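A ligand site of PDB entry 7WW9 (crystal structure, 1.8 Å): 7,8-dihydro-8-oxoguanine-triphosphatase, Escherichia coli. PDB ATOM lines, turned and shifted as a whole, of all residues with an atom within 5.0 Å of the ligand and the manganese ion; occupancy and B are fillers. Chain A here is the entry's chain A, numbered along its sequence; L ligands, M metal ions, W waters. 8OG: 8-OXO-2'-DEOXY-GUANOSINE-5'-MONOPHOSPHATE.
The manganese ion is bound by water W1 (2.1 Å), an oxygen (OP2) of the ligand (2.2 Å), the side-chain carboxylate of Glu 57 (2.2 Å), the backbone carbonyl oxygen of Gly 37 (2.2 Å), water W2 (2.2 Å) and water W3 (2.3 Å).
The manganese ion has six donor atoms within binding distance.
Water W2 lies within hydrogen-bond range of the side-chain carboxylate (OE1) of Glu 57 (2.7 Å), the side-chain carboxylate (OE1) of Glu 34 (2.8 Å), a nitrogen (N2) of the ligand (2.9 Å) and the backbone NH (N) of Gly 37 (3.5 Å).
Water W5 bridges an oxygen (OP1) of the ligand (2.5 Å) and the backbone NH (N) of Lys 39 (2.8 Å).
Water W6 lies within hydrogen-bond range of an oxygen (O3') of the ligand (2.7 Å) and the guanidinium group of Arg 78 (2.8 Å).
The guanidinium group (NH2) of Arg 23 is in hydrogen-bond range of the backbone carbonyl oxygen (O) of His 28 (2.8 Å).
NH1 of Arg 23 lies within salt-bridge range of OE1 of Glu 34 (2.8 Å).
NE of Arg 23 sits at hydrogen-bond distance from O of Met 29 (3.4 Å).
Residues that only touch the ligand: Phe 75, Pro 116, Ile 80, Val 8, Ile 6, Leu 82, Ala 118 and Gly 38.
14 residues have an atom within 4 Å of the ligand: Ile 6, Val 8, Arg 23, His 28, Glu 34, Phe 35, Gly 37, Gly 38, Phe 75, Ile 80, Leu 82, Pro 116, Ala 118 and Asn 119.
Of the 21 residues printed, 2 come within 4 Å of the manganese ion.
A ring nitrogen (ND1) of His 28 sits at hydrogen-bond distance from an oxygen (O3') of the ligand, 2.7 Å away.
OD1 of Asn 119 sits at hydrogen-bond distance from N7 of the ligand (2.9 Å).
The backbone carbonyl oxygen of Phe 35 sits at hydrogen-bond distance from a nitrogen (N1) of the ligand (2.6 Å).
O6 of the ligand is in hydrogen-bond range of N of Phe 35, at 3.1 Å.
The guanidinium group (NH2) of Arg 23 is in salt-bridge range of an oxygen (OP3) of the ligand (2.8 Å).
OE1 of Glu 34 sits at hydrogen-bond distance from N2 of the ligand (3.1 Å).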
ATOM      1  N   ILE A   6      -1.614 -25.655 -20.263  1.00  0.00           N
ATOM      2  CA  ILE A   6      -1.897 -24.278 -19.849  1.00  0.00           C
ATOM      3  C   ILE A   6      -2.314 -24.287 -18.383  1.00  0.00           C
ATOM      4  O   ILE A   6      -3.178 -25.074 -17.983  1.00  0.00           O
ATOM      5  CB  ILE A   6      -3.018 -23.658 -20.702  1.00  0.00           C
ATOM      6  CG1 ILE A   6      -2.669 -23.715 -22.198  1.00  0.00           C
ATOM      7  CG2 ILE A   6      -3.304 -22.212 -20.238  1.00  0.00           C
ATOM      8  CD1 ILE A   6      -1.380 -23.018 -22.565  1.00  0.00           C
ATOM      9  N   VAL A   8      -3.947 -21.830 -15.385  1.00  0.00           N
ATOM     10  CA  VAL A   8      -4.637 -20.570 -15.150  1.00  0.00           C
ATOM     11  C   VAL A   8      -5.095 -20.505 -13.700  1.00  0.00           C
ATOM     12  O   VAL A   8      -5.308 -21.524 -13.032  1.00  0.00           O
ATOM     13  CB  VAL A   8      -5.818 -20.369 -16.118  1.00  0.00           C
ATOM     14  CG1 VAL A   8      -5.370 -20.642 -17.556  1.00  0.00           C
ATOM     15  CG2 VAL A   8      -6.982 -21.263 -15.759  1.00  0.00           C
ATOM     16  N   ARG A  23      -8.498 -10.937 -23.285  1.00  0.00           N
ATOM     17  CA  ARG A  23      -7.411 -11.249 -24.201  1.00  0.00           C
ATOM     18  C   ARG A  23      -7.329 -10.251 -25.354  1.00  0.00           C
ATOM     19  O   ARG A  23      -8.340  -9.704 -25.800  1.00  0.00           O
ATOM     20  CB  ARG A  23      -7.603 -12.677 -24.743  1.00  0.00           C
ATOM     21  CG  ARG A  23      -7.625 -13.682 -23.597  1.00  0.00           C
ATOM     22  CD  ARG A  23      -7.785 -15.116 -24.050  1.00  0.00           C
ATOM     23  NE  ARG A  23      -6.805 -15.532 -25.035  1.00  0.00           N
ATOM     24  CZ  ARG A  23      -5.591 -15.987 -24.743  1.00  0.00           C
ATOM     25  NH1 ARG A  23      -5.186 -16.037 -23.464  1.00  0.00           N
ATOM     26  NH2 ARG A  23      -4.777 -16.369 -25.710  1.00  0.00           N
ATOM     27  N   HIS A  28      -4.812 -15.804 -29.844  1.00  0.00           N
ATOM     28  CA  HIS A  28      -5.760 -16.922 -29.867  1.00  0.00           C
ATOM     29  C   HIS A  28      -6.868 -16.607 -28.863  1.00  0.00           C
ATOM     30  O   HIS A  28      -6.613 -16.016 -27.822  1.00  0.00           O
ATOM     31  CB  HIS A  28      -5.055 -18.233 -29.507  1.00  0.00           C
ATOM     32  CG  HIS A  28      -5.936 -19.434 -29.638  1.00  0.00           C
ATOM     33  ND1 HIS A  28      -6.336 -20.193 -28.555  1.00  0.00           N
ATOM     34  CD2 HIS A  28      -6.529 -19.998 -30.722  1.00  0.00           C
ATOM     35  CE1 HIS A  28      -7.122 -21.166 -28.963  1.00  0.00           C
ATOM     36  NE2 HIS A  28      -7.247 -21.082 -30.271  1.00  0.00           N
ATOM     37  N   MET A  29      -8.093 -17.006 -29.195  1.00  0.00           N
ATOM     38  CA  MET A  29      -9.259 -16.656 -28.398  1.00  0.00           C
ATOM     39  C   MET A  29      -9.293 -15.144 -28.158  1.00  0.00           C
ATOM     40  O   MET A  29      -9.422 -14.653 -27.027  1.00  0.00           O
ATOM     41  CB  MET A  29      -9.279 -17.440 -27.085  1.00  0.00           C
ATOM     42  CG  MET A  29      -9.638 -18.910 -27.276  1.00  0.00           C
ATOM     43  SD  MET A  29     -11.348 -19.050 -27.844  1.00  0.00           S
ATOM     44  CE  MET A  29     -11.132 -19.570 -29.545  1.00  0.00           C
ATOM     45  N   GLU A  34     -11.027 -14.161 -19.575  1.00  0.00           N
ATOM     46  CA  GLU A  34     -10.122 -15.270 -19.297  1.00  0.00           C
ATOM     47  C   GLU A  34      -9.720 -15.226 -17.831  1.00  0.00           C
ATOM     48  O   GLU A  34      -9.710 -14.170 -17.204  1.00  0.00           O
ATOM     49  CB  GLU A  34      -8.863 -15.206 -20.175  1.00  0.00           C
ATOM     50  CG  GLU A  34      -8.099 -13.890 -19.994  1.00  0.00           C
ATOM     51  CD  GLU A  34      -6.657 -13.943 -20.496  1.00  0.00           C
ATOM     52  OE1 GLU A  34      -6.237 -14.996 -21.054  1.00  0.00           O
ATOM     53  OE2 GLU A  34      -5.958 -12.918 -20.327  1.00  0.00           O
ATOM     54  N   PHE A  35      -9.366 -16.397 -17.303  1.00  0.00           N
ATOM     55  CA  PHE A  35      -8.579 -16.452 -16.072  1.00  0.00           C
ATOM     56  C   PHE A  35      -7.112 -16.207 -16.436  1.00  0.00           C
ATOM     57  O   PHE A  35      -6.632 -16.788 -17.413  1.00  0.00           O
ATOM     58  CB  PHE A  35      -8.725 -17.825 -15.401  1.00  0.00           C
ATOM     59  CG  PHE A  35     -10.144 -18.238 -15.165  1.00  0.00           C
ATOM     60  CD1 PHE A  35     -10.988 -17.477 -14.346  1.00  0.00           C
ATOM     61  CD2 PHE A  35     -10.650 -19.398 -15.741  1.00  0.00           C
ATOM     62  CE1 PHE A  35     -12.299 -17.856 -14.121  1.00  0.00           C
ATOM     63  CE2 PHE A  35     -11.950 -19.794 -15.510  1.00  0.00           C
ATOM     64  CZ  PHE A  35     -12.791 -19.021 -14.712  1.00  0.00           C
ATOM     65  N   PRO A  36      -6.384 -15.372 -15.704  1.00  0.00           N
ATOM     66  CA  PRO A  36      -4.963 -15.170 -16.050  1.00  0.00           C
ATOM     67  C   PRO A  36      -4.216 -16.499 -16.022  1.00  0.00           C
ATOM     68  O   PRO A  36      -4.484 -17.363 -15.182  1.00  0.00           O
ATOM     69  CB  PRO A  36      -4.463 -14.227 -14.944  1.00  0.00           C
ATOM     70  CG  PRO A  36      -5.724 -13.473 -14.522  1.00  0.00           C
ATOM     71  CD  PRO A  36      -6.802 -14.538 -14.559  1.00  0.00           C
ATOM     72  N   GLY A  37      -3.302 -16.675 -16.967  1.00  0.00           N
ATOM     73  CA  GLY A  37      -2.515 -17.890 -17.012  1.00  0.00           C
ATOM     74  C   GLY A  37      -1.774 -18.019 -18.330  1.00  0.00           C
ATOM     75  O   GLY A  37      -1.746 -17.078 -19.136  1.00  0.00           O
ATOM     76  N   GLY A  38      -1.148 -19.173 -18.528  1.00  0.00           N
ATOM     77  CA  GLY A  38      -0.361 -19.357 -19.730  1.00  0.00           C
ATOM     78  C   GLY A  38       0.323 -20.710 -19.745  1.00  0.00           C
ATOM     79  O   GLY A  38       0.033 -21.588 -18.924  1.00  0.00           O
ATOM     80  N   LYS A  39       1.236 -20.855 -20.697  1.00  0.00           N
ATOM     81  CA  LYS A  39       1.827 -22.156 -20.993  1.00  0.00           C
ATOM     82  C   LYS A  39       2.756 -22.615 -19.868  1.00  0.00           C
ATOM     83  O   LYS A  39       3.582 -21.832 -19.367  1.00  0.00           O
ATOM     84  CB  LYS A  39       2.594 -22.053 -22.317  1.00  0.00           C
ATOM     85  CG  LYS A  39       3.359 -23.300 -22.723  1.00  0.00           C
ATOM     86  CD  LYS A  39       4.098 -23.040 -24.034  1.00  0.00           C
ATOM     87  CE  LYS A  39       5.264 -23.999 -24.215  1.00  0.00           C
ATOM     88  NZ  LYS A  39       4.813 -25.416 -24.196  1.00  0.00           N
ATOM     89  N   GLU A  53       2.838 -17.359 -13.958  1.00  0.00           N
ATOM     90  CA  GLU A  53       1.941 -16.655 -14.862  1.00  0.00           C
ATOM     91  C   GLU A  53       1.170 -15.555 -14.145  1.00  0.00           C
ATOM     92  O   GLU A  53       0.935 -14.478 -14.715  1.00  0.00           O
ATOM     93  CB  GLU A  53       0.983 -17.636 -15.537  1.00  0.00           C
ATOM     94  CG  GLU A  53       1.652 -18.531 -16.588  1.00  0.00           C
ATOM     95  CD  GLU A  53       2.019 -17.782 -17.867  1.00  0.00           C
ATOM     96  OE1 GLU A  53       1.459 -16.699 -18.111  1.00  0.00           O
ATOM     97  OE2 GLU A  53       2.845 -18.292 -18.645  1.00  0.00           O
ATOM     98  N   GLU A  57       1.351 -11.736 -15.222  1.00  0.00           N
ATOM     99  CA  GLU A  57       0.202 -11.120 -15.867  1.00  0.00           C
ATOM    100  C   GLU A  57      -0.518 -10.129 -14.965  1.00  0.00           C
ATOM    101  O   GLU A  57      -1.011  -9.102 -15.466  1.00  0.00           O
ATOM    102  CB  GLU A  57      -0.765 -12.203 -16.364  1.00  0.00           C
ATOM    103  CG  GLU A  57      -0.180 -13.009 -17.526  1.00  0.00           C
ATOM    104  CD  GLU A  57      -1.224 -13.717 -18.351  1.00  0.00           C
ATOM    105  OE1 GLU A  57      -2.400 -13.744 -17.928  1.00  0.00           O
ATOM    106  OE2 GLU A  57      -0.865 -14.230 -19.421  1.00  0.00           O
ATOM    107  N   PHE A  75      -9.395 -27.170 -29.810  1.00  0.00           N
ATOM    108  CA  PHE A  75      -9.704 -25.998 -30.612  1.00  0.00           C
ATOM    109  C   PHE A  75      -9.530 -26.331 -32.087  1.00  0.00           C
ATOM    110  O   PHE A  75      -8.941 -27.364 -32.442  1.00  0.00           O
ATOM    111  CB  PHE A  75      -8.795 -24.832 -30.207  1.00  0.00           C
ATOM    112  CG  PHE A  75      -9.135 -24.223 -28.882  1.00  0.00           C
ATOM    113  CD1 PHE A  75     -10.189 -23.338 -28.771  1.00  0.00           C
ATOM    114  CD2 PHE A  75      -8.377 -24.515 -27.765  1.00  0.00           C
ATOM    115  CE1 PHE A  75     -10.491 -22.747 -27.535  1.00  0.00           C
ATOM    116  CE2 PHE A  75      -8.679 -23.924 -26.529  1.00  0.00           C
ATOM    117  CZ  PHE A  75      -9.741 -23.041 -26.425  1.00  0.00           C
ATOM    118  N   ARG A  78      -5.540 -26.344 -32.466  1.00  0.00           N
ATOM    119  CA  ARG A  78      -4.630 -26.714 -31.388  1.00  0.00           C
ATOM    120  C   ARG A  78      -5.383 -27.501 -30.332  1.00  0.00           C
ATOM    121  O   ARG A  78      -6.595 -27.352 -30.158  1.00  0.00           O
ATOM    122  CB  ARG A  78      -3.950 -25.474 -30.786  1.00  0.00           C
ATOM    123  CG  ARG A  78      -4.858 -24.563 -29.973  1.00  0.00           C
ATOM    124  CD  ARG A  78      -4.185 -23.196 -29.788  1.00  0.00           C
ATOM    125  NE  ARG A  78      -4.076 -22.496 -31.062  1.00  0.00           N
ATOM    126  CZ  ARG A  78      -3.289 -21.456 -31.286  1.00  0.00           C
ATOM    127  NH1 ARG A  78      -2.519 -20.981 -30.315  1.00  0.00           N
ATOM    128  NH2 ARG A  78      -3.260 -20.879 -32.482  1.00  0.00           N
ATOM    129  N   ILE A  80      -5.296 -28.268 -26.228  1.00  0.00           N
ATOM    130  CA  ILE A  80      -4.688 -27.820 -24.977  1.00  0.00           C
ATOM    131  C   ILE A  80      -5.281 -28.586 -23.802  1.00  0.00           C
ATOM    132  O   ILE A  80      -6.438 -29.012 -23.814  1.00  0.00           O
ATOM    133  CB  ILE A  80      -4.839 -26.304 -24.739  1.00  0.00           C
ATOM    134  CG1 ILE A  80      -6.282 -25.946 -24.417  1.00  0.00           C
ATOM    135  CG2 ILE A  80      -4.303 -25.489 -25.921  1.00  0.00           C
ATOM    136  CD1 ILE A  80      -6.395 -24.557 -23.879  1.00  0.00           C
ATOM    137  N   LEU A  82      -5.936 -27.780 -19.902  1.00  0.00           N
ATOM    138  CA  LEU A  82      -6.087 -26.617 -19.029  1.00  0.00           C
ATOM    139  C   LEU A  82      -6.100 -27.056 -17.584  1.00  0.00           C
ATOM    140  O   LEU A  82      -6.895 -27.929 -17.200  1.00  0.00           O
ATOM    141  CB  LEU A  82      -7.380 -25.862 -19.343  1.00  0.00           C
ATOM    142  CG  LEU A  82      -7.304 -24.915 -20.524  1.00  0.00           C
ATOM    143  CD1 LEU A  82      -8.672 -24.801 -21.167  1.00  0.00           C
ATOM    144  CD2 LEU A  82      -6.838 -23.544 -20.076  1.00  0.00           C
ATOM    145  N   PHE A  84      -7.025 -25.617 -14.107  1.00  0.00           N
ATOM    146  CA  PHE A  84      -7.726 -24.509 -13.462  1.00  0.00           C
ATOM    147  C   PHE A  84      -7.452 -24.557 -11.962  1.00  0.00           C
ATOM    148  O   PHE A  84      -7.981 -25.433 -11.265  1.00  0.00           O
ATOM    149  CB  PHE A  84      -9.235 -24.564 -13.722  1.00  0.00           C
ATOM    150  CG  PHE A  84      -9.614 -24.378 -15.158  1.00  0.00           C
ATOM    151  CD1 PHE A  84      -9.936 -23.108 -15.653  1.00  0.00           C
ATOM    152  CD2 PHE A  84      -9.700 -25.462 -16.019  1.00  0.00           C
ATOM    153  CE1 PHE A  84     -10.322 -22.939 -16.968  1.00  0.00           C
ATOM    154  CE2 PHE A  84     -10.071 -25.299 -17.350  1.00  0.00           C
ATOM    155  CZ  PHE A  84     -10.375 -24.036 -17.832  1.00  0.00           C
ATOM    156  N   PRO A 116     -13.411 -18.479 -23.478  1.00  0.00           N
ATOM    157  CA  PRO A 116     -13.186 -19.582 -24.407  1.00  0.00           C
ATOM    158  C   PRO A 116     -14.113 -20.729 -24.085  1.00  0.00           C
ATOM    159  O   PRO A 116     -14.477 -20.940 -22.919  1.00  0.00           O
ATOM    160  CB  PRO A 116     -11.714 -19.944 -24.177  1.00  0.00           C
ATOM    161  CG  PRO A 116     -11.103 -18.655 -23.696  1.00  0.00           C
ATOM    162  CD  PRO A 116     -12.170 -18.091 -22.800  1.00  0.00           C
ATOM    163  N   ALA A 118     -13.690 -23.773 -23.835  1.00  0.00           N
ATOM    164  CA  ALA A 118     -13.123 -24.747 -22.914  1.00  0.00           C
ATOM    165  C   ALA A 118     -13.509 -24.460 -21.475  1.00  0.00           C
ATOM    166  O   ALA A 118     -13.582 -25.392 -20.664  1.00  0.00           O
ATOM    167  CB  ALA A 118     -11.602 -24.765 -23.061  1.00  0.00           C
ATOM    168  N   ASN A 119     -13.773 -23.190 -21.122  1.00  0.00           N
ATOM    169  CA  ASN A 119     -14.083 -22.822 -19.747  1.00  0.00           C
ATOM    170  C   ASN A 119     -15.526 -23.145 -19.329  1.00  0.00           C
ATOM    171  O   ASN A 119     -15.849 -22.988 -18.140  1.00  0.00           O
ATOM    172  CB  ASN A 119     -13.838 -21.318 -19.522  1.00  0.00           C
ATOM    173  CG  ASN A 119     -12.378 -20.928 -19.692  1.00  0.00           C
ATOM    174  OD1 ASN A 119     -11.613 -21.610 -20.388  1.00  0.00           O
ATOM    175  ND2 ASN A 119     -11.977 -19.847 -19.035  1.00  0.00           N
HETATM  176  OP3 8OG L   1      -2.177 -16.964 -24.807  1.00  0.00           O
HETATM  177  P   8OG L   1      -1.744 -17.663 -23.583  1.00  0.00           P
HETATM  178  OP1 8OG L   1      -0.266 -17.679 -23.505  1.00  0.00           O
HETATM  179  OP2 8OG L   1      -2.295 -17.140 -22.301  1.00  0.00           O
HETATM  180  O5' 8OG L   1      -2.194 -19.207 -23.694  1.00  0.00           O
HETATM  181  C5' 8OG L   1      -3.493 -19.571 -23.249  1.00  0.00           C
HETATM  182  C4' 8OG L   1      -4.115 -20.609 -24.188  1.00  0.00           C
HETATM  183  O4' 8OG L   1      -5.138 -21.322 -23.458  1.00  0.00           O
HETATM  184  C3' 8OG L   1      -4.834 -19.977 -25.368  1.00  0.00           C
HETATM  185  O3' 8OG L   1      -4.888 -20.921 -26.458  1.00  0.00           O
HETATM  186  C2' 8OG L   1      -6.217 -19.696 -24.848  1.00  0.00           C
HETATM  187  C1' 8OG L   1      -6.422 -20.906 -23.955  1.00  0.00           C
HETATM  188  N9  8OG L   1      -7.320 -20.621 -22.818  1.00  0.00           N
HETATM  189  C8  8OG L   1      -8.615 -21.087 -22.624  1.00  0.00           C
HETATM  190  N7  8OG L   1      -9.175 -20.660 -21.577  1.00  0.00           N
HETATM  191  C5  8OG L   1      -8.241 -19.795 -20.973  1.00  0.00           C
HETATM  192  C6  8OG L   1      -8.296 -19.023 -19.760  1.00  0.00           C
HETATM  193  O6  8OG L   1      -9.249 -18.942 -18.983  1.00  0.00           O
HETATM  194  N1  8OG L   1      -7.098 -18.299 -19.535  1.00  0.00           N
HETATM  195  C2  8OG L   1      -5.974 -18.328 -20.372  1.00  0.00           C
HETATM  196  N2  8OG L   1      -4.931 -17.603 -20.024  1.00  0.00           N
HETATM  197  N3  8OG L   1      -5.925 -19.073 -21.505  1.00  0.00           N
HETATM  198  C4  8OG L   1      -7.073 -19.766 -21.750  1.00  0.00           C
HETATM  199  O8  8OG L   1      -9.120 -21.878 -23.429  1.00  0.00           O
HETATM  200 MN    MN M   1      -1.707 -15.680 -20.805  1.00  0.00          MN
HETATM  201  O   HOH W   1       0.246 -16.071 -21.494  1.00  0.00           O
HETATM  202  O   HOH W   2      -3.631 -15.010 -19.993  1.00  0.00           O
HETATM  203  O   HOH W   3      -1.933 -13.868 -22.268  1.00  0.00           O
HETATM  204  O   HOH W   4       1.362 -16.206 -24.935  1.00  0.00           O
HETATM  205  O   HOH W   5       1.710 -18.859 -22.537  1.00  0.00           O
HETATM  206  O   HOH W   6      -2.400 -21.127 -27.485  1.00  0.00           O
HETATM  207  O   HOH W   7      -1.853 -14.474 -24.924  1.00  0.00           O
HETATM  208  O   HOH W   8      -1.742 -18.262 -27.127  1.00  0.00           O
